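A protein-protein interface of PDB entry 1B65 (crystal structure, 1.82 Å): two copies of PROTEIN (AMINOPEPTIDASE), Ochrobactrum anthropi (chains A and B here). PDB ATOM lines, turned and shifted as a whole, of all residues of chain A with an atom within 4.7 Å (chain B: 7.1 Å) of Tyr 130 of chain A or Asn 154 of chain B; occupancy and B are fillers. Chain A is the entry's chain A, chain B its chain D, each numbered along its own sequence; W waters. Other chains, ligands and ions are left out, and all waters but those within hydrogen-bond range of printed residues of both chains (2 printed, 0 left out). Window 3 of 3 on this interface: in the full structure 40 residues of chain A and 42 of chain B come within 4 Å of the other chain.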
ATOM      1  N   PRO A  71       4.937  19.494  25.204  1.00  0.00           N
ATOM      2  CA  PRO A  71       4.547  20.749  25.883  1.00  0.00           C
ATOM      3  C   PRO A  71       5.160  20.793  27.267  1.00  0.00           C
ATOM      4  O   PRO A  71       5.204  19.761  27.949  1.00  0.00           O
ATOM      5  CB  PRO A  71       3.023  20.642  25.986  1.00  0.00           C
ATOM      6  CG  PRO A  71       2.661  19.734  24.838  1.00  0.00           C
ATOM      7  CD  PRO A  71       3.749  18.670  24.925  1.00  0.00           C
ATOM      8  N   LEU A 100       0.104  25.478  29.217  1.00  0.00           N
ATOM      9  CA  LEU A 100       0.954  24.774  28.272  1.00  0.00           C
ATOM     10  C   LEU A 100       0.753  25.422  26.910  1.00  0.00           C
ATOM     11  O   LEU A 100      -0.336  25.919  26.673  1.00  0.00           O
ATOM     12  CB  LEU A 100       0.289  23.379  28.114  1.00  0.00           C
ATOM     13  CG  LEU A 100       0.709  22.128  28.843  1.00  0.00           C
ATOM     14  CD1 LEU A 100       2.029  22.270  29.560  1.00  0.00           C
ATOM     15  CD2 LEU A 100      -0.401  21.557  29.697  1.00  0.00           C
ATOM     16  N   MET A 122      -1.721  22.313  18.199  1.00  0.00           N
ATOM     17  CA  MET A 122      -1.019  21.585  19.271  1.00  0.00           C
ATOM     18  C   MET A 122      -1.169  20.097  19.054  1.00  0.00           C
ATOM     19  O   MET A 122      -0.260  19.321  19.346  1.00  0.00           O
ATOM     20  CB  MET A 122      -1.580  22.045  20.649  1.00  0.00           C
ATOM     21  CG  MET A 122      -0.824  23.350  21.036  1.00  0.00           C
ATOM     22  SD  MET A 122      -1.441  23.984  22.603  1.00  0.00           S
ATOM     23  CE  MET A 122      -0.612  22.809  23.704  1.00  0.00           C
ATOM     24  N   VAL A 123      -2.361  19.638  18.623  1.00  0.00           N
ATOM     25  CA  VAL A 123      -2.569  18.196  18.406  1.00  0.00           C
ATOM     26  C   VAL A 123      -1.631  17.665  17.319  1.00  0.00           C
ATOM     27  O   VAL A 123      -1.055  16.568  17.456  1.00  0.00           O
ATOM     28  CB  VAL A 123      -4.036  17.903  18.095  1.00  0.00           C
ATOM     29  CG1 VAL A 123      -4.288  16.486  17.573  1.00  0.00           C
ATOM     30  CG2 VAL A 123      -4.864  18.136  19.359  1.00  0.00           C
ATOM     31  N   TYR A 126       2.473  18.373  18.690  1.00  0.00           N
ATOM     32  CA  TYR A 126       2.843  17.489  19.796  1.00  0.00           C
ATOM     33  C   TYR A 126       2.064  16.181  19.646  1.00  0.00           C
ATOM     34  O   TYR A 126       1.446  15.642  20.564  1.00  0.00           O
ATOM     35  CB  TYR A 126       2.507  18.186  21.128  1.00  0.00           C
ATOM     36  CG  TYR A 126       3.210  19.522  21.309  1.00  0.00           C
ATOM     37  CD1 TYR A 126       4.591  19.566  21.483  1.00  0.00           C
ATOM     38  CD2 TYR A 126       2.499  20.716  21.290  1.00  0.00           C
ATOM     39  CE1 TYR A 126       5.253  20.757  21.670  1.00  0.00           C
ATOM     40  CE2 TYR A 126       3.139  21.928  21.465  1.00  0.00           C
ATOM     41  CZ  TYR A 126       4.505  21.937  21.645  1.00  0.00           C
ATOM     42  OH  TYR A 126       5.133  23.148  21.804  1.00  0.00           O
ATOM     43  N   ALA A 127       2.083  15.587  18.454  1.00  0.00           N
ATOM     44  CA  ALA A 127       1.379  14.335  18.177  1.00  0.00           C
ATOM     45  C   ALA A 127       1.743  13.210  19.117  1.00  0.00           C
ATOM     46  O   ALA A 127       0.870  12.407  19.510  1.00  0.00           O
ATOM     47  CB  ALA A 127       1.664  13.941  16.724  1.00  0.00           C
ATOM     48  N   SER A 128       2.994  13.062  19.539  1.00  0.00           N
ATOM     49  CA  SER A 128       3.420  12.035  20.464  1.00  0.00           C
ATOM     50  C   SER A 128       2.852  12.237  21.875  1.00  0.00           C
ATOM     51  O   SER A 128       2.980  11.336  22.700  1.00  0.00           O
ATOM     52  CB  SER A 128       4.929  11.932  20.630  1.00  0.00           C
ATOM     53  OG  SER A 128       5.531  13.092  21.145  1.00  0.00           O
ATOM     54  N   THR A 129       2.293  13.407  22.155  1.00  0.00           N
ATOM     55  CA  THR A 129       1.619  13.630  23.436  1.00  0.00           C
ATOM     56  C   THR A 129       0.124  13.391  23.255  1.00  0.00           C
ATOM     57  O   THR A 129      -0.519  12.684  24.028  1.00  0.00           O
ATOM     58  CB  THR A 129       1.869  15.069  23.939  1.00  0.00           C
ATOM     59  OG1 THR A 129       3.278  15.220  24.228  1.00  0.00           O
ATOM     60  CG2 THR A 129       1.077  15.418  25.183  1.00  0.00           C
ATOM     61  N   TYR A 130      -0.494  14.086  22.303  1.00  0.00           N
ATOM     62  CA  TYR A 130      -1.945  14.103  22.151  1.00  0.00           C
ATOM     63  C   TYR A 130      -2.580  13.068  21.245  1.00  0.00           C
ATOM     64  O   TYR A 130      -3.767  12.790  21.446  1.00  0.00           O
ATOM     65  CB  TYR A 130      -2.380  15.515  21.663  1.00  0.00           C
ATOM     66  CG  TYR A 130      -2.036  16.570  22.696  1.00  0.00           C
ATOM     67  CD1 TYR A 130      -2.657  16.597  23.930  1.00  0.00           C
ATOM     68  CD2 TYR A 130      -1.085  17.562  22.403  1.00  0.00           C
ATOM     69  CE1 TYR A 130      -2.315  17.572  24.874  1.00  0.00           C
ATOM     70  CE2 TYR A 130      -0.756  18.519  23.338  1.00  0.00           C
ATOM     71  CZ  TYR A 130      -1.369  18.528  24.571  1.00  0.00           C
ATOM     72  OH  TYR A 130      -1.064  19.492  25.523  1.00  0.00           O
ATOM     73  N   GLN A 131      -1.855  12.469  20.309  1.00  0.00           N
ATOM     74  CA  GLN A 131      -2.481  11.462  19.430  1.00  0.00           C
ATOM     75  C   GLN A 131      -2.140  10.081  19.970  1.00  0.00           C
ATOM     76  O   GLN A 131      -1.398   9.265  19.430  1.00  0.00           O
ATOM     77  CB  GLN A 131      -2.046  11.668  17.986  1.00  0.00           C
ATOM     78  CG  GLN A 131      -2.291  13.055  17.444  1.00  0.00           C
ATOM     79  CD  GLN A 131      -2.052  13.291  15.983  1.00  0.00           C
ATOM     80  OE1 GLN A 131      -1.549  14.337  15.535  1.00  0.00           O
ATOM     81  NE2 GLN A 131      -2.408  12.312  15.156  1.00  0.00           N
ATOM     82  N   THR A 132      -2.629   9.833  21.176  1.00  0.00           N
ATOM     83  CA  THR A 132      -2.375   8.660  21.975  1.00  0.00           C
ATOM     84  C   THR A 132      -3.657   8.221  22.674  1.00  0.00           C
ATOM     85  O   THR A 132      -4.688   8.873  22.530  1.00  0.00           O
ATOM     86  CB  THR A 132      -1.351   8.923  23.102  1.00  0.00           C
ATOM     87  OG1 THR A 132      -1.906   9.924  23.985  1.00  0.00           O
ATOM     88  CG2 THR A 132       0.013   9.334  22.592  1.00  0.00           C
ATOM     89  N   LEU A 136      -6.351  13.455  27.476  1.00  0.00           N
ATOM     90  CA  LEU A 136      -5.765  14.778  27.705  1.00  0.00           C
ATOM     91  C   LEU A 136      -6.641  15.846  27.064  1.00  0.00           C
ATOM     92  O   LEU A 136      -7.302  15.592  26.054  1.00  0.00           O
ATOM     93  CB  LEU A 136      -4.417  14.846  26.982  1.00  0.00           C
ATOM     94  CG  LEU A 136      -3.100  14.489  27.653  1.00  0.00           C
ATOM     95  CD1 LEU A 136      -3.179  13.931  29.050  1.00  0.00           C
ATOM     96  CD2 LEU A 136      -2.224  13.670  26.710  1.00  0.00           C
ATOM     97  N   ILE A 138      -6.758  20.221  26.082  1.00  0.00           N
ATOM     98  CA  ILE A 138      -5.921  21.399  25.863  1.00  0.00           C
ATOM     99  C   ILE A 138      -6.756  22.654  26.094  1.00  0.00           C
ATOM    100  O   ILE A 138      -7.851  22.757  25.544  1.00  0.00           O
ATOM    101  CB  ILE A 138      -5.430  21.377  24.399  1.00  0.00           C
ATOM    102  CG1 ILE A 138      -4.662  20.090  24.083  1.00  0.00           C
ATOM    103  CG2 ILE A 138      -4.614  22.641  24.114  1.00  0.00           C
ATOM    104  CD1 ILE A 138      -4.295  19.933  22.601  1.00  0.00           C
ATOM    105  N   MET A 303       4.467  17.048  31.970  1.00  0.00           N
ATOM    106  CA  MET A 303       3.052  17.288  32.158  1.00  0.00           C
ATOM    107  C   MET A 303       2.576  16.389  33.321  1.00  0.00           C
ATOM    108  O   MET A 303       3.268  15.449  33.725  1.00  0.00           O
ATOM    109  CB  MET A 303       2.267  16.946  30.890  1.00  0.00           C
ATOM    110  CG  MET A 303       2.609  17.946  29.770  1.00  0.00           C
ATOM    111  SD  MET A 303       1.970  17.360  28.169  1.00  0.00           S
ATOM    112  CE  MET A 303       0.214  17.512  28.419  1.00  0.00           C
ATOM    113  N   ARG B  51     -10.977   9.131  10.303  1.00  0.00           N
ATOM    114  CA  ARG B  51     -10.949   9.044  11.762  1.00  0.00           C
ATOM    115  C   ARG B  51     -11.076   7.580  12.154  1.00  0.00           C
ATOM    116  O   ARG B  51     -11.491   6.773  11.310  1.00  0.00           O
ATOM    117  CB  ARG B  51     -12.099   9.867  12.367  1.00  0.00           C
ATOM    118  CG  ARG B  51     -12.167  11.291  11.848  1.00  0.00           C
ATOM    119  CD  ARG B  51     -10.895  12.077  12.139  1.00  0.00           C
ATOM    120  NE  ARG B  51     -10.499  12.009  13.537  1.00  0.00           N
ATOM    121  CZ  ARG B  51      -9.358  12.366  14.084  1.00  0.00           C
ATOM    122  NH1 ARG B  51      -8.356  12.830  13.325  1.00  0.00           N
ATOM    123  NH2 ARG B  51      -9.200  12.241  15.392  1.00  0.00           N
ATOM    124  N   ARG B  53     -12.405   6.816  15.497  1.00  0.00           N
ATOM    125  CA  ARG B  53     -13.444   6.752  16.531  1.00  0.00           C
ATOM    126  C   ARG B  53     -14.661   7.561  16.094  1.00  0.00           C
ATOM    127  O   ARG B  53     -14.530   8.548  15.371  1.00  0.00           O
ATOM    128  CB  ARG B  53     -12.885   7.308  17.846  1.00  0.00           C
ATOM    129  CG  ARG B  53     -11.559   6.709  18.276  1.00  0.00           C
ATOM    130  CD  ARG B  53     -11.032   7.268  19.580  1.00  0.00           C
ATOM    131  NE  ARG B  53     -12.054   7.315  20.618  1.00  0.00           N
ATOM    132  CZ  ARG B  53     -12.222   8.308  21.491  1.00  0.00           C
ATOM    133  NH1 ARG B  53     -11.424   9.367  21.480  1.00  0.00           N
ATOM    134  NH2 ARG B  53     -13.201   8.190  22.365  1.00  0.00           N
ATOM    135  N   ASN B 107     -18.061  20.453  24.024  1.00  0.00           N
ATOM    136  CA  ASN B 107     -16.948  19.607  24.488  1.00  0.00           C
ATOM    137  C   ASN B 107     -15.696  20.491  24.531  1.00  0.00           C
ATOM    138  O   ASN B 107     -15.671  21.566  23.927  1.00  0.00           O
ATOM    139  CB  ASN B 107     -16.758  18.406  23.567  1.00  0.00           C
ATOM    140  CG  ASN B 107     -16.197  18.735  22.199  1.00  0.00           C
ATOM    141  OD1 ASN B 107     -15.015  19.038  22.024  1.00  0.00           O
ATOM    142  ND2 ASN B 107     -17.025  18.687  21.152  1.00  0.00           N
ATOM    143  N   HIS B 109     -12.682  20.648  23.189  1.00  0.00           N
ATOM    144  CA  HIS B 109     -11.990  21.174  22.029  1.00  0.00           C
ATOM    145  C   HIS B 109     -12.920  21.833  21.028  1.00  0.00           C
ATOM    146  O   HIS B 109     -12.384  22.321  20.039  1.00  0.00           O
ATOM    147  CB  HIS B 109     -11.172  20.042  21.357  1.00  0.00           C
ATOM    148  CG  HIS B 109     -10.041  19.563  22.201  1.00  0.00           C
ATOM    149  ND1 HIS B 109      -9.638  20.145  23.387  1.00  0.00           N
ATOM    150  CD2 HIS B 109      -9.248  18.479  22.029  1.00  0.00           C
ATOM    151  CE1 HIS B 109      -8.619  19.449  23.925  1.00  0.00           C
ATOM    152  NE2 HIS B 109      -8.368  18.451  23.097  1.00  0.00           N
ATOM    153  N   TYR B 146     -15.341  17.390  29.149  1.00  0.00           N
ATOM    154  CA  TYR B 146     -14.546  16.563  28.247  1.00  0.00           C
ATOM    155  C   TYR B 146     -15.170  15.212  27.912  1.00  0.00           C
ATOM    156  O   TYR B 146     -15.255  14.352  28.794  1.00  0.00           O
ATOM    157  CB  TYR B 146     -13.175  16.397  28.953  1.00  0.00           C
ATOM    158  CG  TYR B 146     -12.218  15.463  28.223  1.00  0.00           C
ATOM    159  CD1 TYR B 146     -11.504  15.922  27.134  1.00  0.00           C
ATOM    160  CD2 TYR B 146     -12.045  14.149  28.665  1.00  0.00           C
ATOM    161  CE1 TYR B 146     -10.606  15.081  26.464  1.00  0.00           C
ATOM    162  CE2 TYR B 146     -11.161  13.298  27.995  1.00  0.00           C
ATOM    163  CZ  TYR B 146     -10.457  13.783  26.922  1.00  0.00           C
ATOM    164  OH  TYR B 146      -9.560  12.997  26.208  1.00  0.00           O
ATOM    165  N   GLY B 148     -13.841  12.966  25.639  1.00  0.00           N
ATOM    166  CA  GLY B 148     -12.865  12.142  24.916  1.00  0.00           C
ATOM    167  C   GLY B 148     -12.979  10.638  25.132  1.00  0.00           C
ATOM    168  O   GLY B 148     -12.461   9.937  24.225  1.00  0.00           O
ATOM    169  N   ASN B 151     -16.178  10.206  22.662  1.00  0.00           N
ATOM    170  CA  ASN B 151     -16.181  10.986  21.425  1.00  0.00           C
ATOM    171  C   ASN B 151     -14.816  11.114  20.805  1.00  0.00           C
ATOM    172  O   ASN B 151     -13.807  11.130  21.512  1.00  0.00           O
ATOM    173  CB  ASN B 151     -16.770  12.390  21.754  1.00  0.00           C
ATOM    174  CG  ASN B 151     -16.728  13.385  20.633  1.00  0.00           C
ATOM    175  OD1 ASN B 151     -17.117  13.085  19.503  1.00  0.00           O
ATOM    176  ND2 ASN B 151     -16.306  14.623  20.890  1.00  0.00           N
ATOM    177  N   ASP B 152     -14.707  11.281  19.495  1.00  0.00           N
ATOM    178  CA  ASP B 152     -13.478  11.557  18.759  1.00  0.00           C
ATOM    179  C   ASP B 152     -13.187  13.052  18.918  1.00  0.00           C
ATOM    180  O   ASP B 152     -13.287  13.868  18.004  1.00  0.00           O
ATOM    181  CB  ASP B 152     -13.736  11.247  17.266  1.00  0.00           C
ATOM    182  CG  ASP B 152     -12.525  11.452  16.378  1.00  0.00           C
ATOM    183  OD1 ASP B 152     -11.426  11.203  16.894  1.00  0.00           O
ATOM    184  OD2 ASP B 152     -12.642  11.861  15.198  1.00  0.00           O
ATOM    185  N   ILE B 153     -12.764  13.459  20.128  1.00  0.00           N
ATOM    186  CA  ILE B 153     -12.663  14.873  20.458  1.00  0.00           C
ATOM    187  C   ILE B 153     -11.566  15.579  19.657  1.00  0.00           C
ATOM    188  O   ILE B 153     -11.704  16.747  19.363  1.00  0.00           O
ATOM    189  CB  ILE B 153     -12.459  15.023  21.988  1.00  0.00           C
ATOM    190  CG1 ILE B 153     -12.692  16.490  22.382  1.00  0.00           C
ATOM    191  CG2 ILE B 153     -11.096  14.509  22.400  1.00  0.00           C
ATOM    192  CD1 ILE B 153     -12.666  16.657  23.905  1.00  0.00           C
ATOM    193  N   ASN B 154     -10.527  14.861  19.231  1.00  0.00           N
ATOM    194  CA  ASN B 154      -9.496  15.476  18.398  1.00  0.00           C
ATOM    195  C   ASN B 154      -9.814  15.414  16.920  1.00  0.00           C
ATOM    196  O   ASN B 154      -8.973  15.796  16.092  1.00  0.00           O
ATOM    197  CB  ASN B 154      -8.118  14.851  18.688  1.00  0.00           C
ATOM    198  CG  ASN B 154      -7.655  15.250  20.082  1.00  0.00           C
ATOM    199  OD1 ASN B 154      -8.067  16.287  20.595  1.00  0.00           O
ATOM    200  ND2 ASN B 154      -6.810  14.445  20.690  1.00  0.00           N
ATOM    201  N   GLY B 155     -11.024  15.047  16.540  1.00  0.00           N
ATOM    202  CA  GLY B 155     -11.488  15.113  15.171  1.00  0.00           C
ATOM    203  C   GLY B 155     -12.327  16.367  14.971  1.00  0.00           C
ATOM    204  O   GLY B 155     -12.869  16.602  13.898  1.00  0.00           O
ATOM    205  N   PHE B 156     -12.553  17.143  16.035  1.00  0.00           N
ATOM    206  CA  PHE B 156     -13.360  18.357  15.991  1.00  0.00           C
ATOM    207  C   PHE B 156     -14.664  18.188  15.231  1.00  0.00           C
ATOM    208  O   PHE B 156     -14.949  18.934  14.278  1.00  0.00           O
ATOM    209  CB  PHE B 156     -12.520  19.472  15.321  1.00  0.00           C
ATOM    210  CG  PHE B 156     -11.239  19.701  16.075  1.00  0.00           C
ATOM    211  CD1 PHE B 156     -11.220  20.606  17.140  1.00  0.00           C
ATOM    212  CD2 PHE B 156     -10.077  19.014  15.788  1.00  0.00           C
ATOM    213  CE1 PHE B 156     -10.067  20.826  17.849  1.00  0.00           C
ATOM    214  CE2 PHE B 156      -8.907  19.193  16.510  1.00  0.00           C
ATOM    215  CZ  PHE B 156      -8.917  20.122  17.548  1.00  0.00           C
ATOM    216  N   PRO B 157     -15.549  17.313  15.656  1.00  0.00           N
ATOM    217  CA  PRO B 157     -16.816  17.094  14.988  1.00  0.00           C
ATOM    218  C   PRO B 157     -17.791  18.252  15.000  1.00  0.00           C
ATOM    219  O   PRO B 157     -18.649  18.299  14.110  1.00  0.00           O
ATOM    220  CB  PRO B 157     -17.403  15.870  15.699  1.00  0.00           C
ATOM    221  CG  PRO B 157     -16.701  15.776  17.018  1.00  0.00           C
ATOM    222  CD  PRO B 157     -15.337  16.364  16.784  1.00  0.00           C
HETATM  223  O   HOH W   1      -8.242  13.734  24.118  1.00  0.00           O
HETATM  224  O   HOH W   2      -6.015  14.922  23.584  1.00  0.00           O
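O of Leu 136 of chain A lies close to OH of Tyr 146 of chain B, at 3.4 Å.
No position is printed for both chains.
Of the 4 pairs that touch across the chains among the printed residues, none has its exchanged pair printed and touching as well.
Tyr 126 of chain A touches none of the printed residues of chain B.
Ala 127 of chain A touches none of the printed residues of chain B.
Tyr 130 of chain A touches just one residue of chain B: Asn 154.
Printed residues of chain B within 4 Å of Leu 136 of chain A: Tyr 146.
Printed residues of chain B within 4 Å of Ile 138 of chain A: His 109.
Of the printed residues of chain A, Tyr 146 of chain B touches Leu 136 (3.4 Å).
Asn 154 of chain B touches just these residues of chain A: Val 123 and Tyr 130.
The nearest residue of chain B that does not touch Tyr 130 of chain A is His 109 of chain B (6.1 Å).
The nearest printed residue of chain B that does not touch Leu 136 of chain A is His 109 of chain B (4.2 Å).
The backbone carbonyl oxygen (O) of Val 123 of chain A sits close to the side-chain amide oxygen (OE1) of Gln 131 of chain A (3.0 Å).
OD1 of Asn 107 of chain B sits at hydrogen-bond distance from N of His 109 of chain B (3.1 Å).
The side-chain amide oxygen of Asn 154 of chain B sits close to a ring nitrogen (NE2) of His 109 of chain B, 3.3 Å away.
Water W1 bridges OH of Tyr 146 of chain B (2.6 Å) and O of Leu 136 of chain A (2.8 Å).
Water W2 bridges the backbone carbonyl oxygen of Leu 136 of chain A (2.9 Å) and the side-chain amide nitrogen of Asn 154 of chain B (3.0 Å).
Among the printed residues, pairs that only touch across the chains: Ile 138 of chain A with His 109 of chain B, Tyr 130 of chain A with Asn 154 of chain B and Val 123 of chain A with Asn 154 of chain B.
Of the 13 printed residues of chain B, 3 touch a printed residue of chain A.
Of the 14 printed residues of chain A, 4 touch a printed residue of chain B.
Hydrophobic or aromatic side chains of chain A within 4 Å of the printed part of chain B: Val 123 and Ile 138.
Among the printed residues, no Asp or Glu carboxylate lies within 4 Å of a Lys or Arg side-chain nitrogen of the other chain.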
